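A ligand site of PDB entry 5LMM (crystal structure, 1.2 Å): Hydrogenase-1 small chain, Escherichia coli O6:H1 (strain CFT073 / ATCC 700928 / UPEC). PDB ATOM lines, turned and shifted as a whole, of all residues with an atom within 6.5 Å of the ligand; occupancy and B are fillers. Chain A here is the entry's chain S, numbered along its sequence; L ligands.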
ATOM      1  N   ILE A 186     -11.607  13.596  14.678  1.00  0.00           N
ATOM      2  CA  ILE A 186     -12.221  12.285  14.820  1.00  0.00           C
ATOM      3  C   ILE A 186     -12.053  11.776  16.249  1.00  0.00           C
ATOM      4  O   ILE A 186     -12.994  11.271  16.885  1.00  0.00           O
ATOM      5  CB  ILE A 186     -11.628  11.263  13.768  1.00  0.00           C
ATOM      6  CG1 ILE A 186     -11.994  11.689  12.345  1.00  0.00           C
ATOM      7  CG2 ILE A 186     -11.984   9.824  14.083  1.00  0.00           C
ATOM      8  CD1 ILE A 186     -13.428  11.590  12.032  1.00  0.00           C
ATOM      9  N   HIS A 187     -10.824  11.847  16.753  1.00  0.00           N
ATOM     10  CA  HIS A 187     -10.430  11.343  18.086  1.00  0.00           C
ATOM     11  C   HIS A 187     -11.069  12.084  19.232  1.00  0.00           C
ATOM     12  O   HIS A 187     -11.080  11.545  20.329  1.00  0.00           O
ATOM     13  CB  HIS A 187      -8.891  11.433  18.131  1.00  0.00           C
ATOM     14  CG  HIS A 187      -8.167  10.980  19.357  1.00  0.00           C
ATOM     15  ND1 HIS A 187      -7.944   9.654  19.682  1.00  0.00           N
ATOM     16  CD2 HIS A 187      -7.387  11.708  20.182  1.00  0.00           C
ATOM     17  CE1 HIS A 187      -7.126   9.608  20.721  1.00  0.00           C
ATOM     18  NE2 HIS A 187      -6.770  10.842  21.038  1.00  0.00           N
ATOM     19  N   ASP A 188     -11.577  13.294  18.993  1.00  0.00           N
ATOM     20  CA  ASP A 188     -12.217  14.015  20.071  1.00  0.00           C
ATOM     21  C   ASP A 188     -13.712  13.641  20.224  1.00  0.00           C
ATOM     22  O   ASP A 188     -14.343  14.084  21.164  1.00  0.00           O
ATOM     23  CB  ASP A 188     -11.878  15.496  19.943  1.00  0.00           C
ATOM     24  CG  ASP A 188     -10.404  15.803  20.324  1.00  0.00           C
ATOM     25  OD1 ASP A 188      -9.758  15.031  21.121  1.00  0.00           O
ATOM     26  OD2 ASP A 188      -9.893  16.844  19.854  1.00  0.00           O
ATOM     27  N   CYS A 190     -14.556  10.095  19.364  1.00  0.00           N
ATOM     28  CA  CYS A 190     -14.460   8.668  19.051  1.00  0.00           C
ATOM     29  C   CYS A 190     -14.937   7.829  20.234  1.00  0.00           C
ATOM     30  O   CYS A 190     -14.472   7.963  21.368  1.00  0.00           O
ATOM     31  CB  CYS A 190     -13.030   8.288  18.706  1.00  0.00           C
ATOM     32  SG  CYS A 190     -12.914   6.502  18.245  1.00  0.00           S
ATOM     33  N   TYR A 191     -15.851   6.901  19.952  1.00  0.00           N
ATOM     34  CA  TYR A 191     -16.423   6.013  20.966  1.00  0.00           C
ATOM     35  C   TYR A 191     -15.433   5.031  21.552  1.00  0.00           C
ATOM     36  O   TYR A 191     -15.750   4.396  22.547  1.00  0.00           O
ATOM     37  CB  TYR A 191     -17.716   5.333  20.484  1.00  0.00           C
ATOM     38  CG  TYR A 191     -17.477   4.098  19.622  1.00  0.00           C
ATOM     39  CD1 TYR A 191     -16.644   4.068  18.497  1.00  0.00           C
ATOM     40  CD2 TYR A 191     -18.124   2.921  19.974  1.00  0.00           C
ATOM     41  CE1 TYR A 191     -16.496   2.894  17.801  1.00  0.00           C
ATOM     42  CE2 TYR A 191     -17.930   1.740  19.291  1.00  0.00           C
ATOM     43  CZ  TYR A 191     -17.082   1.719  18.193  1.00  0.00           C
ATOM     44  OH  TYR A 191     -16.803   0.581  17.508  1.00  0.00           O
ATOM     45  N   ARG A 192     -14.230   4.892  20.965  1.00  0.00           N
ATOM     46  CA  ARG A 192     -13.192   4.036  21.537  1.00  0.00           C
ATOM     47  C   ARG A 192     -12.217   4.825  22.431  1.00  0.00           C
ATOM     48  O   ARG A 192     -11.247   4.242  22.930  1.00  0.00           O
ATOM     49  CB  ARG A 192     -12.463   3.224  20.463  1.00  0.00           C
ATOM     50  CG  ARG A 192     -13.402   2.307  19.708  1.00  0.00           C
ATOM     51  CD  ARG A 192     -12.708   1.377  18.752  1.00  0.00           C
ATOM     52  NE  ARG A 192     -13.661   0.556  18.034  1.00  0.00           N
ATOM     53  CZ  ARG A 192     -13.385  -0.602  17.437  1.00  0.00           C
ATOM     54  NH1 ARG A 192     -12.188  -1.171  17.523  1.00  0.00           N
ATOM     55  NH2 ARG A 192     -14.372  -1.215  16.775  1.00  0.00           N
ATOM     56  N   ARG A 193     -12.492   6.099  22.667  1.00  0.00           N
ATOM     57  CA  ARG A 193     -11.568   6.912  23.453  1.00  0.00           C
ATOM     58  C   ARG A 193     -11.327   6.365  24.848  1.00  0.00           C
ATOM     59  O   ARG A 193     -10.220   6.423  25.338  1.00  0.00           O
ATOM     60  CB  ARG A 193     -12.012   8.353  23.477  1.00  0.00           C
ATOM     61  CG  ARG A 193     -11.028   9.286  24.113  1.00  0.00           C
ATOM     62  CD  ARG A 193      -9.767   9.387  23.267  1.00  0.00           C
ATOM     63  NE  ARG A 193      -8.925  10.257  24.025  1.00  0.00           N
ATOM     64  CZ  ARG A 193      -8.787  11.548  23.812  1.00  0.00           C
ATOM     65  NH1 ARG A 193      -9.342  12.145  22.773  1.00  0.00           N
ATOM     66  NH2 ARG A 193      -8.035  12.249  24.650  1.00  0.00           N
ATOM     67  N   ALA A 194     -12.356   5.805  25.482  1.00  0.00           N
ATOM     68  CA  ALA A 194     -12.173   5.201  26.796  1.00  0.00           C
ATOM     69  C   ALA A 194     -11.010   4.225  26.801  1.00  0.00           C
ATOM     70  O   ALA A 194     -10.256   4.122  27.780  1.00  0.00           O
ATOM     71  CB  ALA A 194     -13.430   4.471  27.242  1.00  0.00           C
ATOM     72  N   HIS A 195     -10.946   3.437  25.735  1.00  0.00           N
ATOM     73  CA  HIS A 195      -9.867   2.432  25.612  1.00  0.00           C
ATOM     74  C   HIS A 195      -8.521   3.096  25.422  1.00  0.00           C
ATOM     75  O   HIS A 195      -7.525   2.687  26.065  1.00  0.00           O
ATOM     76  CB  HIS A 195     -10.186   1.427  24.537  1.00  0.00           C
ATOM     77  CG  HIS A 195     -11.492   0.724  24.746  1.00  0.00           C
ATOM     78  ND1 HIS A 195     -11.757  -0.015  25.869  1.00  0.00           N
ATOM     79  CD2 HIS A 195     -12.594   0.616  23.963  1.00  0.00           C
ATOM     80  CE1 HIS A 195     -12.989  -0.519  25.787  1.00  0.00           C
ATOM     81  NE2 HIS A 195     -13.481  -0.218  24.603  1.00  0.00           N
ATOM     82  N   PHE A 196      -8.442   4.104  24.560  1.00  0.00           N
ATOM     83  CA  PHE A 196      -7.188   4.852  24.404  1.00  0.00           C
ATOM     84  C   PHE A 196      -6.738   5.348  25.771  1.00  0.00           C
ATOM     85  O   PHE A 196      -5.543   5.193  26.132  1.00  0.00           O
ATOM     86  CB  PHE A 196      -7.438   6.030  23.444  1.00  0.00           C
ATOM     87  CG  PHE A 196      -6.240   6.925  23.240  1.00  0.00           C
ATOM     88  CD1 PHE A 196      -5.362   6.658  22.199  1.00  0.00           C
ATOM     89  CD2 PHE A 196      -6.026   7.999  24.029  1.00  0.00           C
ATOM     90  CE1 PHE A 196      -4.272   7.461  21.998  1.00  0.00           C
ATOM     91  CE2 PHE A 196      -4.962   8.862  23.785  1.00  0.00           C
ATOM     92  CZ  PHE A 196      -4.063   8.586  22.788  1.00  0.00           C
ATOM     93  N   PHE A 201      -5.540  -1.468  23.771  1.00  0.00           N
ATOM     94  CA  PHE A 201      -5.287  -1.347  22.354  1.00  0.00           C
ATOM     95  C   PHE A 201      -5.350  -2.702  21.658  1.00  0.00           C
ATOM     96  O   PHE A 201      -4.836  -3.708  22.159  1.00  0.00           O
ATOM     97  CB  PHE A 201      -3.874  -0.785  22.134  1.00  0.00           C
ATOM     98  CG  PHE A 201      -3.657   0.582  22.700  1.00  0.00           C
ATOM     99  CD1 PHE A 201      -4.335   1.658  22.195  1.00  0.00           C
ATOM    100  CD2 PHE A 201      -2.768   0.806  23.747  1.00  0.00           C
ATOM    101  CE1 PHE A 201      -4.133   2.920  22.700  1.00  0.00           C
ATOM    102  CE2 PHE A 201      -2.565   2.067  24.251  1.00  0.00           C
ATOM    103  CZ  PHE A 201      -3.254   3.148  23.724  1.00  0.00           C
ATOM    104  N   TYR A 214     -11.451  -2.500  21.205  1.00  0.00           N
ATOM    105  CA  TYR A 214     -10.442  -1.636  21.750  1.00  0.00           C
ATOM    106  C   TYR A 214      -9.913  -0.637  20.720  1.00  0.00           C
ATOM    107  O   TYR A 214     -10.141  -0.718  19.518  1.00  0.00           O
ATOM    108  CB  TYR A 214      -9.319  -2.462  22.385  1.00  0.00           C
ATOM    109  CG  TYR A 214      -9.661  -3.084  23.744  1.00  0.00           C
ATOM    110  CD1 TYR A 214     -10.937  -3.040  24.312  1.00  0.00           C
ATOM    111  CD2 TYR A 214      -8.649  -3.742  24.445  1.00  0.00           C
ATOM    112  CE1 TYR A 214     -11.218  -3.652  25.553  1.00  0.00           C
ATOM    113  CE2 TYR A 214      -8.910  -4.285  25.696  1.00  0.00           C
ATOM    114  CZ  TYR A 214     -10.192  -4.258  26.231  1.00  0.00           C
ATOM    115  OH  TYR A 214     -10.394  -4.841  27.450  1.00  0.00           O
ATOM    116  N   CYS A 215      -9.156   0.343  21.230  1.00  0.00           N
ATOM    117  CA  CYS A 215      -8.630   1.424  20.417  1.00  0.00           C
ATOM    118  C   CYS A 215      -7.636   0.910  19.401  1.00  0.00           C
ATOM    119  O   CYS A 215      -6.866  -0.031  19.653  1.00  0.00           O
ATOM    120  CB  CYS A 215      -8.029   2.482  21.329  1.00  0.00           C
ATOM    121  SG  CYS A 215      -7.042   3.790  20.528  1.00  0.00           S
ATOM    122  N   LEU A 216      -7.638   1.594  18.240  1.00  0.00           N
ATOM    123  CA  LEU A 216      -6.834   1.255  17.049  1.00  0.00           C
ATOM    124  C   LEU A 216      -5.577   2.077  16.889  1.00  0.00           C
ATOM    125  O   LEU A 216      -4.900   1.964  15.833  1.00  0.00           O
ATOM    126  CB  LEU A 216      -7.749   1.332  15.808  1.00  0.00           C
ATOM    127  CG  LEU A 216      -8.913   0.342  15.860  1.00  0.00           C
ATOM    128  CD1 LEU A 216      -9.912   0.594  14.762  1.00  0.00           C
ATOM    129  CD2 LEU A 216      -8.535  -1.094  15.845  1.00  0.00           C
ATOM    130  N   TYR A 217      -5.221   2.834  17.906  1.00  0.00           N
ATOM    131  CA  TYR A 217      -3.994   3.660  17.839  1.00  0.00           C
ATOM    132  C   TYR A 217      -2.746   2.880  17.433  1.00  0.00           C
ATOM    133  O   TYR A 217      -1.970   3.362  16.570  1.00  0.00           O
ATOM    134  CB  TYR A 217      -3.807   4.325  19.192  1.00  0.00           C
ATOM    135  CG  TYR A 217      -2.501   5.029  19.370  1.00  0.00           C
ATOM    136  CD1 TYR A 217      -2.214   6.204  18.717  1.00  0.00           C
ATOM    137  CD2 TYR A 217      -1.490   4.470  20.185  1.00  0.00           C
ATOM    138  CE1 TYR A 217      -0.970   6.825  18.860  1.00  0.00           C
ATOM    139  CE2 TYR A 217      -0.248   5.068  20.323  1.00  0.00           C
ATOM    140  CZ  TYR A 217       0.012   6.252  19.635  1.00  0.00           C
ATOM    141  OH  TYR A 217       1.159   6.844  19.757  1.00  0.00           O
ATOM    142  N   LYS A 218      -2.507   1.757  18.056  1.00  0.00           N
ATOM    143  CA  LYS A 218      -1.306   0.936  17.750  1.00  0.00           C
ATOM    144  C   LYS A 218      -1.400   0.256  16.410  1.00  0.00           C
ATOM    145  O   LYS A 218      -0.368  -0.221  15.895  1.00  0.00           O
ATOM    146  CB  LYS A 218      -0.984  -0.062  18.895  1.00  0.00           C
ATOM    147  CG  LYS A 218      -0.621   0.608  20.175  1.00  0.00           C
ATOM    148  CD  LYS A 218      -0.046  -0.361  21.198  1.00  0.00           C
ATOM    149  CE  LYS A 218       0.448   0.423  22.377  1.00  0.00           C
ATOM    150  NZ  LYS A 218       0.891  -0.501  23.449  1.00  0.00           N
ATOM    151  N   CYS A 221      -4.173   4.108  13.580  1.00  0.00           N
ATOM    152  CA  CYS A 221      -5.269   5.075  13.459  1.00  0.00           C
ATOM    153  C   CYS A 221      -4.793   6.514  13.446  1.00  0.00           C
ATOM    154  O   CYS A 221      -4.084   6.944  14.369  1.00  0.00           O
ATOM    155  CB  CYS A 221      -6.216   4.887  14.663  1.00  0.00           C
ATOM    156  SG  CYS A 221      -7.707   5.901  14.508  1.00  0.00           S
ATOM    157  N   LYS A 222      -5.237   7.258  12.437  1.00  0.00           N
ATOM    158  CA  LYS A 222      -4.884   8.682  12.317  1.00  0.00           C
ATOM    159  C   LYS A 222      -5.979   9.611  12.831  1.00  0.00           C
ATOM    160  O   LYS A 222      -5.914  10.821  12.627  1.00  0.00           O
ATOM    161  CB  LYS A 222      -4.508   9.029  10.869  1.00  0.00           C
ATOM    162  CG  LYS A 222      -3.285   8.177  10.367  1.00  0.00           C
ATOM    163  CD  LYS A 222      -2.111   8.189  11.376  1.00  0.00           C
ATOM    164  CE  LYS A 222      -0.835   7.530  10.964  1.00  0.00           C
ATOM    165  NZ  LYS A 222      -0.971   6.183  10.391  1.00  0.00           N
ATOM    166  N   GLY A 223      -6.956   9.045  13.550  1.00  0.00           N
ATOM    167  CA  GLY A 223      -7.973   9.893  14.152  1.00  0.00           C
ATOM    168  C   GLY A 223      -7.466  11.074  15.006  1.00  0.00           C
ATOM    169  O   GLY A 223      -8.048  12.162  14.932  1.00  0.00           O
ATOM    170  N   PRO A 224      -6.339  10.885  15.704  1.00  0.00           N
ATOM    171  CA  PRO A 224      -5.833  11.997  16.512  1.00  0.00           C
ATOM    172  C   PRO A 224      -5.355  13.248  15.740  1.00  0.00           C
ATOM    173  O   PRO A 224      -5.221  14.299  16.365  1.00  0.00           O
ATOM    174  CB  PRO A 224      -4.643  11.386  17.291  1.00  0.00           C
ATOM    175  CG  PRO A 224      -5.040   9.964  17.427  1.00  0.00           C
ATOM    176  CD  PRO A 224      -5.660   9.623  16.072  1.00  0.00           C
ATOM    177  N   PHE A 241     -18.580   3.626  10.714  1.00  0.00           N
ATOM    178  CA  PHE A 241     -17.483   4.448  10.189  1.00  0.00           C
ATOM    179  C   PHE A 241     -16.242   3.553  10.243  1.00  0.00           C
ATOM    180  O   PHE A 241     -16.288   2.475  10.835  1.00  0.00           O
ATOM    181  CB  PHE A 241     -17.340   5.806  10.903  1.00  0.00           C
ATOM    182  CG  PHE A 241     -16.771   5.817  12.302  1.00  0.00           C
ATOM    183  CD1 PHE A 241     -17.461   5.293  13.382  1.00  0.00           C
ATOM    184  CD2 PHE A 241     -15.549   6.464  12.534  1.00  0.00           C
ATOM    185  CE1 PHE A 241     -16.958   5.420  14.694  1.00  0.00           C
ATOM    186  CE2 PHE A 241     -15.078   6.572  13.844  1.00  0.00           C
ATOM    187  CZ  PHE A 241     -15.774   6.015  14.915  1.00  0.00           C
ATOM    188  N   ILE A 243     -13.452   3.184  11.973  1.00  0.00           N
ATOM    189  CA  ILE A 243     -13.020   2.666  13.284  1.00  0.00           C
ATOM    190  C   ILE A 243     -14.056   1.708  13.849  1.00  0.00           C
ATOM    191  O   ILE A 243     -13.711   0.703  14.443  1.00  0.00           O
ATOM    192  CB  ILE A 243     -12.745   3.856  14.190  1.00  0.00           C
ATOM    193  CG1 ILE A 243     -11.455   4.592  13.799  1.00  0.00           C
ATOM    194  CG2 ILE A 243     -12.683   3.476  15.697  1.00  0.00           C
ATOM    195  CD1 ILE A 243     -11.427   6.070  14.092  1.00  0.00           C
ATOM    196  N   GLY A 248      -8.321   1.443  11.600  1.00  0.00           N
ATOM    197  CA  GLY A 248      -7.997   2.821  11.968  1.00  0.00           C
ATOM    198  C   GLY A 248      -8.333   3.800  10.862  1.00  0.00           C
ATOM    199  O   GLY A 248      -8.330   3.480   9.679  1.00  0.00           O
ATOM    200  N   CYS A 249      -8.602   5.017  11.271  1.00  0.00           N
ATOM    201  CA  CYS A 249      -8.683   6.137  10.320  1.00  0.00           C
ATOM    202  C   CYS A 249      -7.374   6.205   9.512  1.00  0.00           C
ATOM    203  O   CYS A 249      -6.291   6.089  10.072  1.00  0.00           O
ATOM    204  CB  CYS A 249      -8.916   7.417  11.112  1.00  0.00           C
ATOM    205  SG  CYS A 249      -8.969   8.990  10.213  1.00  0.00           S
HETATM  206 FE1  LIG L   1      -8.344   5.194  19.284  1.00  0.00          FE
HETATM  207 FE2  LIG L   1      -8.427   6.128  16.694  1.00  0.00          FE
HETATM  208 FE3  LIG L   1      -8.486   7.856  18.806  1.00  0.00          FE
HETATM  209 FE4  LIG L   1     -10.630   6.307  18.274  1.00  0.00          FE
HETATM  210  S1  LIG L   1      -9.763   7.977  16.923  1.00  0.00           S
HETATM  211  S2  LIG L   1      -9.722   6.657  20.345  1.00  0.00           S
HETATM  212  S3  LIG L   1      -9.636   4.336  17.590  1.00  0.00           S
HETATM  213  S4  LIG L   1      -6.735   6.502  18.200  1.00  0.00           S
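SG of Cys 221 is bound to FE2 of the ligand (2.3 Å).
An iron atom (FE1) of the ligand is bound by the side-chain sulfur of Cys 215 (2.3 Å).
The backbone NH (N) of Arg 193 lies close to a sulfur (S2) of the ligand, at 3.7 Å.
ND1 of His 187 binds FE3 of the ligand (2.1 Å).
The backbone NH (N) of Leu 216 sits close to a sulfur (S3) of the ligand (3.5 Å).
An iron atom (FE4) of the ligand is bound by the side-chain sulfur (SG) of Cys 190 (2.3 Å).
Merely in contact with the ligand: Arg 192, Phe 196, Tyr 217, Gly 223, Pro 224 and Ile 243.
Within 4 Å of the ligand: His 187, Cys 190, Arg 192, Arg 193, Phe 196, Cys 215, Leu 216, Tyr 217, Cys 221, Gly 223, Pro 224 and Ile 243.
The nearest printed residue that does not touch the ligand is Ile 186 (4.1 Å).
The guanidinium group (NH1) of Arg 193 sits at hydrogen-bond distance from the backbone carbonyl oxygen (O) of His 187 (3.1 Å).
The backbone NH (N) of Cys 221 sits at hydrogen-bond distance from the backbone carbonyl oxygen (O) of Leu 216, at 3.2 Å.
NH1 of Arg 193 lies within salt-bridge range of OD1 of Asp 188, 3.4 Å away.
SG of Cys 190 sits close to N of Arg 192 (3.4 Å).
The backbone NH (N) of His 187 lies within hydrogen-bond range of the backbone carbonyl oxygen (O) of Gly 223 (3.3 Å).
The guanidinium group (NH1) of Arg 192 sits at hydrogen-bond distance from the backbone carbonyl oxygen (O) of Tyr 214, at 2.9 Å.
SG of Cys 221 lies close to N of Gly 223, 3.4 Å away.
SG of Cys 221 sits close to N of Cys 249, 3.5 Å away.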
